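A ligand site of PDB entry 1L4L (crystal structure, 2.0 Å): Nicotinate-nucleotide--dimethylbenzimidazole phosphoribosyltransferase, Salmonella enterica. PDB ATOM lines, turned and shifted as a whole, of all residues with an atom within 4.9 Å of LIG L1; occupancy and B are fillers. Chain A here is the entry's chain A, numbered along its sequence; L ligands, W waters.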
ATOM      1  N   VAL A  77     -21.356  -9.650   3.699  1.00  0.00           N
ATOM      2  CA  VAL A  77     -21.248  -9.606   5.160  1.00  0.00           C
ATOM      3  C   VAL A  77     -19.935 -10.212   5.669  1.00  0.00           C
ATOM      4  O   VAL A  77     -19.714 -10.264   6.879  1.00  0.00           O
ATOM      5  CB  VAL A  77     -22.428 -10.365   5.840  1.00  0.00           C
ATOM      6  CG1 VAL A  77     -23.759  -9.674   5.534  1.00  0.00           C
ATOM      7  CG2 VAL A  77     -22.465 -11.815   5.368  1.00  0.00           C
ATOM      8  N   ALA A  78     -19.068 -10.642   4.750  1.00  0.00           N
ATOM      9  CA  ALA A  78     -17.780 -11.242   5.119  1.00  0.00           C
ATOM     10  C   ALA A  78     -16.656 -10.815   4.183  1.00  0.00           C
ATOM     11  O   ALA A  78     -16.838 -10.784   2.967  1.00  0.00           O
ATOM     12  CB  ALA A  78     -17.904 -12.779   5.112  1.00  0.00           C
ATOM     13  N   GLU A 174     -16.616 -25.227  14.058  1.00  0.00           N
ATOM     14  CA  GLU A 174     -17.123 -24.991  12.717  1.00  0.00           C
ATOM     15  C   GLU A 174     -16.122 -24.254  11.834  1.00  0.00           C
ATOM     16  O   GLU A 174     -15.070 -23.790  12.293  1.00  0.00           O
ATOM     17  CB  GLU A 174     -18.430 -24.189  12.773  1.00  0.00           C
ATOM     18  CG  GLU A 174     -18.420 -23.016  13.738  1.00  0.00           C
ATOM     19  CD  GLU A 174     -17.246 -22.081  13.527  1.00  0.00           C
ATOM     20  OE1 GLU A 174     -17.145 -21.459  12.441  1.00  0.00           O
ATOM     21  OE2 GLU A 174     -16.405 -21.970  14.430  1.00  0.00           O
ATOM     22  N   LEU A 175     -16.460 -24.177  10.553  1.00  0.00           N
ATOM     23  CA  LEU A 175     -15.663 -23.514   9.560  1.00  0.00           C
ATOM     24  C   LEU A 175     -16.642 -23.156   8.428  1.00  0.00           C
ATOM     25  O   LEU A 175     -17.253 -24.033   7.809  1.00  0.00           O
ATOM     26  CB  LEU A 175     -14.565 -24.454   9.041  1.00  0.00           C
ATOM     27  CG  LEU A 175     -13.674 -23.950   7.907  1.00  0.00           C
ATOM     28  CD1 LEU A 175     -12.902 -22.717   8.424  1.00  0.00           C
ATOM     29  CD2 LEU A 175     -12.684 -25.029   7.454  1.00  0.00           C
ATOM     30  N   GLY A 176     -16.807 -21.871   8.165  1.00  0.00           N
ATOM     31  CA  GLY A 176     -17.703 -21.450   7.106  1.00  0.00           C
ATOM     32  C   GLY A 176     -17.708 -19.938   7.009  1.00  0.00           C
ATOM     33  O   GLY A 176     -18.128 -19.258   7.945  1.00  0.00           O
ATOM     34  N   MET A 177     -17.245 -19.404   5.878  1.00  0.00           N
ATOM     35  CA  MET A 177     -17.206 -17.968   5.712  1.00  0.00           C
ATOM     36  C   MET A 177     -18.618 -17.408   5.760  1.00  0.00           C
ATOM     37  O   MET A 177     -19.537 -17.982   5.168  1.00  0.00           O
ATOM     38  CB  MET A 177     -16.539 -17.604   4.381  1.00  0.00           C
ATOM     39  CG  MET A 177     -15.137 -18.201   4.203  1.00  0.00           C
ATOM     40  SD  MET A 177     -13.993 -17.799   5.557  1.00  0.00           S
ATOM     41  CE  MET A 177     -13.908 -19.392   6.442  1.00  0.00           C
ATOM     42  N   ALA A 178     -18.773 -16.314   6.499  1.00  0.00           N
ATOM     43  CA  ALA A 178     -20.030 -15.612   6.695  1.00  0.00           C
ATOM     44  C   ALA A 178     -20.932 -16.218   7.767  1.00  0.00           C
ATOM     45  O   ALA A 178     -22.035 -15.701   7.987  1.00  0.00           O
ATOM     46  CB  ALA A 178     -20.825 -15.524   5.364  1.00  0.00           C
ATOM     47  N   ASN A 179     -20.501 -17.279   8.448  1.00  0.00           N
ATOM     48  CA  ASN A 179     -21.407 -17.866   9.431  1.00  0.00           C
ATOM     49  C   ASN A 179     -21.725 -17.064  10.697  1.00  0.00           C
ATOM     50  O   ASN A 179     -22.618 -17.448  11.448  1.00  0.00           O
ATOM     51  CB  ASN A 179     -21.028 -19.345   9.766  1.00  0.00           C
ATOM     52  CG  ASN A 179     -19.732 -19.491  10.562  1.00  0.00           C
ATOM     53  OD1 ASN A 179     -19.086 -18.526  10.974  1.00  0.00           O
ATOM     54  ND2 ASN A 179     -19.350 -20.756  10.790  1.00  0.00           N
ATOM     55  N   THR A 180     -21.049 -15.952  10.946  1.00  0.00           N
ATOM     56  CA  THR A 180     -21.409 -15.186  12.144  1.00  0.00           C
ATOM     57  C   THR A 180     -22.702 -14.391  11.870  1.00  0.00           C
ATOM     58  O   THR A 180     -23.311 -13.821  12.779  1.00  0.00           O
ATOM     59  CB  THR A 180     -20.296 -14.231  12.627  1.00  0.00           C
ATOM     60  OG1 THR A 180     -19.998 -13.261  11.620  1.00  0.00           O
ATOM     61  CG2 THR A 180     -19.030 -15.014  12.977  1.00  0.00           C
ATOM     62  N   THR A 181     -23.130 -14.343  10.607  1.00  0.00           N
ATOM     63  CA  THR A 181     -24.367 -13.644  10.278  1.00  0.00           C
ATOM     64  C   THR A 181     -25.572 -14.523  10.677  1.00  0.00           C
ATOM     65  O   THR A 181     -26.455 -14.058  11.410  1.00  0.00           O
ATOM     66  CB  THR A 181     -24.413 -13.247   8.800  1.00  0.00           C
ATOM     67  OG1 THR A 181     -23.446 -12.216   8.578  1.00  0.00           O
ATOM     68  CG2 THR A 181     -25.793 -12.705   8.412  1.00  0.00           C
ATOM     69  N   ILE A 201     -18.086  -8.141  14.496  1.00  0.00           N
ATOM     70  CA  ILE A 201     -17.234  -7.976  13.329  1.00  0.00           C
ATOM     71  C   ILE A 201     -16.774  -9.298  12.701  1.00  0.00           C
ATOM     72  O   ILE A 201     -16.057  -9.304  11.707  1.00  0.00           O
ATOM     73  CB  ILE A 201     -15.979  -7.158  13.653  1.00  0.00           C
ATOM     74  CG1 ILE A 201     -15.125  -7.896  14.686  1.00  0.00           C
ATOM     75  CG2 ILE A 201     -16.366  -5.781  14.157  1.00  0.00           C
ATOM     76  CD1 ILE A 201     -13.733  -7.370  14.827  1.00  0.00           C
ATOM     77  N   GLY A 202     -17.198 -10.431  13.278  1.00  0.00           N
ATOM     78  CA  GLY A 202     -16.805 -11.718  12.732  1.00  0.00           C
ATOM     79  C   GLY A 202     -15.311 -11.800  12.469  1.00  0.00           C
ATOM     80  O   GLY A 202     -14.513 -11.491  13.355  1.00  0.00           O
ATOM     81  N   ALA A 203     -14.927 -12.215  11.265  1.00  0.00           N
ATOM     82  CA  ALA A 203     -13.517 -12.322  10.927  1.00  0.00           C
ATOM     83  C   ALA A 203     -13.013 -11.012  10.304  1.00  0.00           C
ATOM     84  O   ALA A 203     -12.898 -10.865   9.082  1.00  0.00           O
ATOM     85  CB  ALA A 203     -13.269 -13.505   9.959  1.00  0.00           C
ATOM     86  N   LYS A 213     -24.387  -5.511   7.616  1.00  0.00           N
ATOM     87  CA  LYS A 213     -24.563  -6.811   8.248  1.00  0.00           C
ATOM     88  C   LYS A 213     -25.810  -6.770   9.149  1.00  0.00           C
ATOM     89  O   LYS A 213     -26.598  -7.708   9.138  1.00  0.00           O
ATOM     90  CB  LYS A 213     -23.317  -7.179   9.059  1.00  0.00           C
ATOM     91  CG  LYS A 213     -23.280  -8.604   9.584  1.00  0.00           C
ATOM     92  CD  LYS A 213     -21.890  -8.923  10.092  1.00  0.00           C
ATOM     93  CE  LYS A 213     -21.834 -10.231  10.846  1.00  0.00           C
ATOM     94  NZ  LYS A 213     -20.454 -10.468  11.394  1.00  0.00           N
ATOM     95  N   ASP A 263     -17.499 -23.997  22.042  1.00  0.00           N
ATOM     96  CA  ASP A 263     -16.360 -23.238  21.548  1.00  0.00           C
ATOM     97  C   ASP A 263     -16.693 -21.758  21.683  1.00  0.00           C
ATOM     98  O   ASP A 263     -16.791 -21.252  22.803  1.00  0.00           O
ATOM     99  CB  ASP A 263     -16.055 -23.602  20.072  1.00  0.00           C
ATOM    100  CG  ASP A 263     -14.800 -22.886  19.522  1.00  0.00           C
ATOM    101  OD1 ASP A 263     -13.889 -22.550  20.308  1.00  0.00           O
ATOM    102  OD2 ASP A 263     -14.708 -22.667  18.296  1.00  0.00           O
ATOM    103  N   GLY A 264     -16.867 -21.058  20.574  1.00  0.00           N
ATOM    104  CA  GLY A 264     -17.188 -19.638  20.634  1.00  0.00           C
ATOM    105  C   GLY A 264     -18.609 -19.237  20.257  1.00  0.00           C
ATOM    106  O   GLY A 264     -19.552 -20.006  20.434  1.00  0.00           O
ATOM    107  N   PHE A 265     -18.754 -18.030  19.720  1.00  0.00           N
ATOM    108  CA  PHE A 265     -20.053 -17.482  19.330  1.00  0.00           C
ATOM    109  C   PHE A 265     -20.921 -18.384  18.459  1.00  0.00           C
ATOM    110  O   PHE A 265     -22.129 -18.501  18.708  1.00  0.00           O
ATOM    111  CB  PHE A 265     -19.877 -16.121  18.650  1.00  0.00           C
ATOM    112  CG  PHE A 265     -21.167 -15.374  18.427  1.00  0.00           C
ATOM    113  CD1 PHE A 265     -21.636 -15.113  17.140  1.00  0.00           C
ATOM    114  CD2 PHE A 265     -21.914 -14.913  19.501  1.00  0.00           C
ATOM    115  CE1 PHE A 265     -22.824 -14.397  16.926  1.00  0.00           C
ATOM    116  CE2 PHE A 265     -23.101 -14.202  19.307  1.00  0.00           C
ATOM    117  CZ  PHE A 265     -23.556 -13.944  18.020  1.00  0.00           C
ATOM    118  N   LEU A 266     -20.341 -19.022  17.444  1.00  0.00           N
ATOM    119  CA  LEU A 266     -21.144 -19.896  16.587  1.00  0.00           C
ATOM    120  C   LEU A 266     -21.701 -21.048  17.422  1.00  0.00           C
ATOM    121  O   LEU A 266     -22.869 -21.421  17.274  1.00  0.00           O
ATOM    122  CB  LEU A 266     -20.337 -20.450  15.407  1.00  0.00           C
ATOM    123  CG  LEU A 266     -19.812 -19.504  14.324  1.00  0.00           C
ATOM    124  CD1 LEU A 266     -20.847 -18.433  13.987  1.00  0.00           C
ATOM    125  CD2 LEU A 266     -18.516 -18.828  14.789  1.00  0.00           C
ATOM    126  N   SER A 291     -15.986 -15.779  23.968  1.00  0.00           N
ATOM    127  CA  SER A 291     -15.742 -15.209  22.638  1.00  0.00           C
ATOM    128  C   SER A 291     -15.698 -13.688  22.593  1.00  0.00           C
ATOM    129  O   SER A 291     -16.510 -13.005  23.238  1.00  0.00           O
ATOM    130  CB  SER A 291     -16.791 -15.685  21.643  1.00  0.00           C
ATOM    131  OG  SER A 291     -16.607 -15.050  20.382  1.00  0.00           O
ATOM    132  N   GLU A 293     -16.596 -11.990  20.207  1.00  0.00           N
ATOM    133  CA  GLU A 293     -17.688 -11.523  19.370  1.00  0.00           C
ATOM    134  C   GLU A 293     -18.639 -10.679  20.230  1.00  0.00           C
ATOM    135  O   GLU A 293     -18.914 -11.029  21.384  1.00  0.00           O
ATOM    136  CB  GLU A 293     -18.412 -12.724  18.755  1.00  0.00           C
ATOM    137  CG  GLU A 293     -19.467 -12.394  17.723  1.00  0.00           C
ATOM    138  CD  GLU A 293     -18.898 -11.971  16.379  1.00  0.00           C
ATOM    139  OE1 GLU A 293     -19.706 -11.726  15.472  1.00  0.00           O
ATOM    140  OE2 GLU A 293     -17.665 -11.867  16.198  1.00  0.00           O
ATOM    141  N   MET A 313     -10.481 -14.746  22.270  1.00  0.00           N
ATOM    142  CA  MET A 313     -10.365 -15.481  21.027  1.00  0.00           C
ATOM    143  C   MET A 313     -11.610 -15.346  20.164  1.00  0.00           C
ATOM    144  O   MET A 313     -12.726 -15.167  20.670  1.00  0.00           O
ATOM    145  CB  MET A 313     -10.038 -16.947  21.315  1.00  0.00           C
ATOM    146  CG  MET A 313      -8.571 -17.188  21.622  1.00  0.00           C
ATOM    147  SD  MET A 313      -8.292 -18.701  22.568  1.00  0.00           S
ATOM    148  CE  MET A 313      -8.793 -19.934  21.395  1.00  0.00           C
ATOM    149  N   ARG A 314     -11.410 -15.429  18.857  1.00  0.00           N
ATOM    150  CA  ARG A 314     -12.498 -15.298  17.895  1.00  0.00           C
ATOM    151  C   ARG A 314     -12.116 -15.969  16.573  1.00  0.00           C
ATOM    152  O   ARG A 314     -12.436 -15.472  15.487  1.00  0.00           O
ATOM    153  CB  ARG A 314     -12.809 -13.809  17.652  1.00  0.00           C
ATOM    154  CG  ARG A 314     -11.596 -12.959  17.247  1.00  0.00           C
ATOM    155  CD  ARG A 314     -12.006 -11.496  17.085  1.00  0.00           C
ATOM    156  NE  ARG A 314     -10.899 -10.572  16.885  1.00  0.00           N
ATOM    157  CZ  ARG A 314     -10.209 -10.439  15.748  1.00  0.00           C
ATOM    158  NH1 ARG A 314     -10.519 -11.174  14.686  1.00  0.00           N
ATOM    159  NH2 ARG A 314      -9.235  -9.549  15.669  1.00  0.00           N
ATOM    160  N   LEU A 315     -11.429 -17.093  16.666  1.00  0.00           N
ATOM    161  CA  LEU A 315     -11.027 -17.834  15.482  1.00  0.00           C
ATOM    162  C   LEU A 315     -12.093 -18.836  15.069  1.00  0.00           C
ATOM    163  O   LEU A 315     -12.406 -18.978  13.892  1.00  0.00           O
ATOM    164  CB  LEU A 315      -9.720 -18.594  15.753  1.00  0.00           C
ATOM    165  CG  LEU A 315      -9.285 -19.625  14.688  1.00  0.00           C
ATOM    166  CD1 LEU A 315      -8.941 -18.953  13.367  1.00  0.00           C
ATOM    167  CD2 LEU A 315      -8.069 -20.397  15.206  1.00  0.00           C
ATOM    168  N   GLY A 316     -12.645 -19.541  16.053  1.00  0.00           N
ATOM    169  CA  GLY A 316     -13.625 -20.565  15.764  1.00  0.00           C
ATOM    170  C   GLY A 316     -12.851 -21.869  15.578  1.00  0.00           C
ATOM    171  O   GLY A 316     -11.773 -22.033  16.154  1.00  0.00           O
ATOM    172  N   GLU A 317     -13.405 -22.787  14.783  1.00  0.00           N
ATOM    173  CA  GLU A 317     -12.800 -24.090  14.481  1.00  0.00           C
ATOM    174  C   GLU A 317     -12.841 -25.074  15.649  1.00  0.00           C
ATOM    175  O   GLU A 317     -12.472 -26.242  15.500  1.00  0.00           O
ATOM    176  CB  GLU A 317     -11.323 -23.938  14.075  1.00  0.00           C
ATOM    177  CG  GLU A 317     -11.026 -22.935  12.983  1.00  0.00           C
ATOM    178  CD  GLU A 317      -9.563 -22.998  12.561  1.00  0.00           C
ATOM    179  OE1 GLU A 317      -8.838 -23.831  13.127  1.00  0.00           O
ATOM    180  OE2 GLU A 317      -9.149 -22.224  11.670  1.00  0.00           O
HETATM  181  P1  LIG L   1     -17.339 -14.192   9.266  1.00  0.00           P
HETATM  182  O1  LIG L   1     -18.804 -14.228   9.533  1.00  0.00           O
HETATM  183  O2  LIG L   1     -16.843 -12.782   9.260  1.00  0.00           O
HETATM  184  O3  LIG L   1     -17.013 -14.887   7.839  1.00  0.00           O
HETATM  185  O4  LIG L   1     -16.588 -14.989  10.403  1.00  0.00           O
HETATM  186  C1  LIG L   1     -16.936 -16.363  10.616  1.00  0.00           C
HETATM  187  C2  LIG L   1     -15.708 -17.193  10.454  1.00  0.00           C
HETATM  188  O5  LIG L   1     -14.700 -16.717  11.389  1.00  0.00           O
HETATM  189  C3  LIG L   1     -15.899 -18.668  10.710  1.00  0.00           C
HETATM  190  O6  LIG L   1     -15.211 -19.538   9.783  1.00  0.00           O
HETATM  191  C4  LIG L   1     -15.461 -18.803  12.200  1.00  0.00           C
HETATM  192  O7  LIG L   1     -14.659 -20.015  12.320  1.00  0.00           O
HETATM  193  C5  LIG L   1     -14.680 -17.518  12.534  1.00  0.00           C
HETATM  194  N1  LIG L   1     -15.147 -16.717  13.744  1.00  0.00           N
HETATM  195  C6  LIG L   1     -15.318 -15.289  13.687  1.00  0.00           C
HETATM  196  C7  LIG L   1     -15.726 -14.707  14.898  1.00  0.00           C
HETATM  197  C8  LIG L   1     -15.963 -15.384  16.132  1.00  0.00           C
HETATM  198  C9  LIG L   1     -15.746 -16.841  16.037  1.00  0.00           C
HETATM  199  C10 LIG L   1     -15.339 -17.482  14.864  1.00  0.00           C
HETATM  200  C11 LIG L   1     -16.027 -17.437  17.423  1.00  0.00           C
HETATM  201  O8  LIG L   1     -16.361 -16.864  18.424  1.00  0.00           O
HETATM  202  O9  LIG L   1     -15.834 -18.770  17.357  1.00  0.00           O
HETATM  203  C1  LG2 L   2     -10.522 -19.158   9.430  1.00  0.00           C
HETATM  204  C2  LG2 L   2     -11.388 -18.105   9.083  1.00  0.00           C
HETATM  205  C3  LG2 L   2     -11.014 -17.194   8.172  1.00  0.00           C
HETATM  206  C4  LG2 L   2      -9.794 -17.281   7.580  1.00  0.00           C
HETATM  207  C5  LG2 L   2      -8.947 -18.323   7.931  1.00  0.00           C
HETATM  208  C6  LG2 L   2      -9.323 -19.252   8.858  1.00  0.00           C
HETATM  209  N1  LG2 L   2     -10.910 -20.168  10.402  1.00  0.00           N
HETATM  210  C7  LG2 L   2      -7.590 -18.428   7.289  1.00  0.00           C
HETATM  211  C8  LG2 L   2     -12.743 -17.985   9.718  1.00  0.00           C
HETATM  212  O   HOH W   1     -18.467 -10.544   9.226  1.00  0.00           O
HETATM  213  O   HOH W   2     -14.894 -13.586   6.595  1.00  0.00           O
HETATM  214  O   HOH W   3     -15.122 -11.485  16.087  1.00  0.00           O
HETATM  215  O   HOH W   4     -15.398 -11.226   7.485  1.00  0.00           O
HETATM  216  O   HOH W   5     -14.019 -19.879  19.078  1.00  0.00           O
HETATM  217  O   HOH W   6     -17.720 -20.827  17.862  1.00  0.00           O
HETATM  218  O   HOH W   7     -20.656 -12.750   8.264  1.00  0.00           O
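An oxygen (O1) of LIG L1 lies within hydrogen-bond range of the backbone NH (N) of Thr 180, 3.2 Å away.
O1 of LIG L1 lies within hydrogen-bond range of OG1 of Thr 180.
The backbone NH (N) of Ala 178 is in hydrogen-bond range of an oxygen (O3) of LIG L1 (2.6 Å).
The side-chain hydroxyl of Ser 291 sits at hydrogen-bond distance from an oxygen (O8) of LIG L1, 2.7 Å away.
N of Ala 203 is in hydrogen-bond range of O2 of LIG L1 (2.8 Å).
The side-chain carboxylate (OE1) of Glu 174 sits at hydrogen-bond distance from an oxygen (O7) of LIG L1 (2.9 Å).
The backbone carbonyl oxygen of Leu 315 lies within hydrogen-bond range of an oxygen (O7) of LIG L1, at 2.9 Å.
The backbone NH (N) of Phe 265 sits at hydrogen-bond distance from an oxygen (O8) of LIG L1 (3.0 Å).
O6 of LIG L1 is in hydrogen-bond range of N of Gly 176.
An oxygen (O6) of LIG L1 sits at hydrogen-bond distance from the backbone carbonyl oxygen (O) of Gly 176.
The side-chain carboxylate (OE2) of Glu 317 sits at hydrogen-bond distance from a nitrogen (N1) of LG2 L2 (3.0 Å).
NZ of Lys 213 sits at hydrogen-bond distance from OG1 of Thr 180 (2.8 Å).
The side-chain hydroxyl of Ser 291 sits close to the backbone NH of Glu 293, 3.1 Å away.
The side-chain carboxylate (OE1) of Glu 174 lies within hydrogen-bond range of the side-chain amide nitrogen (ND2) of Asn 179 (2.8 Å).
The side-chain carboxylate (OE2) of Glu 174 lies within hydrogen-bond range of the backbone NH (N) of Glu 317, at 3.1 Å.
The side-chain amide oxygen (OD1) of Asn 179 sits close to the backbone carbonyl oxygen (O) of Gly 176 (3.3 Å).
The backbone NH (N) of Gly 202 sits at hydrogen-bond distance from the side-chain carboxylate (OE2) of Glu 293, at 3.3 Å.
The backbone carbonyl oxygen (O) of Arg 314 lies close to a nitrogen (N1) of LIG L1, at 3.5 Å.
Ala 78 touches LIG L1.
Met 177 touches LIG L1 (CE to O6, 3.6 Å).
Asn 179 touches LIG L1.
Gly 202 touches LIG L1 (CA to O2, 3.6 Å).
Gly 264 touches LIG L1.
Leu 266 touches LIG L1.
Glu 293 touches LIG L1 (OE2 to C7, 3.7 Å).
Gly 316 touches LIG L1 (CA to O9, 3.3 Å).
Glu 317 touches LIG L1 (N to O7, 3.9 Å).
Water W7 lies within hydrogen-bond range of an oxygen (O1) of LIG L1 (2.7 Å), the side-chain hydroxyl (OG1) of Thr 181 (2.9 Å), the backbone carbonyl oxygen (O) of Val 77 (3.0 Å), the backbone carbonyl oxygen (O) of Ala 178 (3.3 Å) and the side-chain hydroxyl (OG1) of Thr 180 (3.5 Å).
Water W5 lies within hydrogen-bond range of an oxygen (O9) of LIG L1 (2.7 Å), the side-chain carboxylate (OD1) of Asp 263 (2.9 Å), the backbone NH (N) of Gly 316 (3.3 Å) and the backbone NH (N) of Gly 264 (3.4 Å).
Water W1 lies within hydrogen-bond range of the backbone carbonyl oxygen (O) of Val 77, an oxygen (O2) of LIG L1 and the side-chain amino group (NZ) of Lys 213.
Water W4 bridges O2 of LIG L1 (2.8 Å) and O of Ala 203 (3.0 Å).
Water W6 lies within hydrogen-bond range of an oxygen (O9) of LIG L1 (2.8 Å), the backbone NH of Gly 264 (2.9 Å) and the backbone NH of Leu 266 (3.2 Å).
Water W3 bridges OE2 of Glu 293 (2.6 Å) and O of Gly 202 (2.8 Å).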
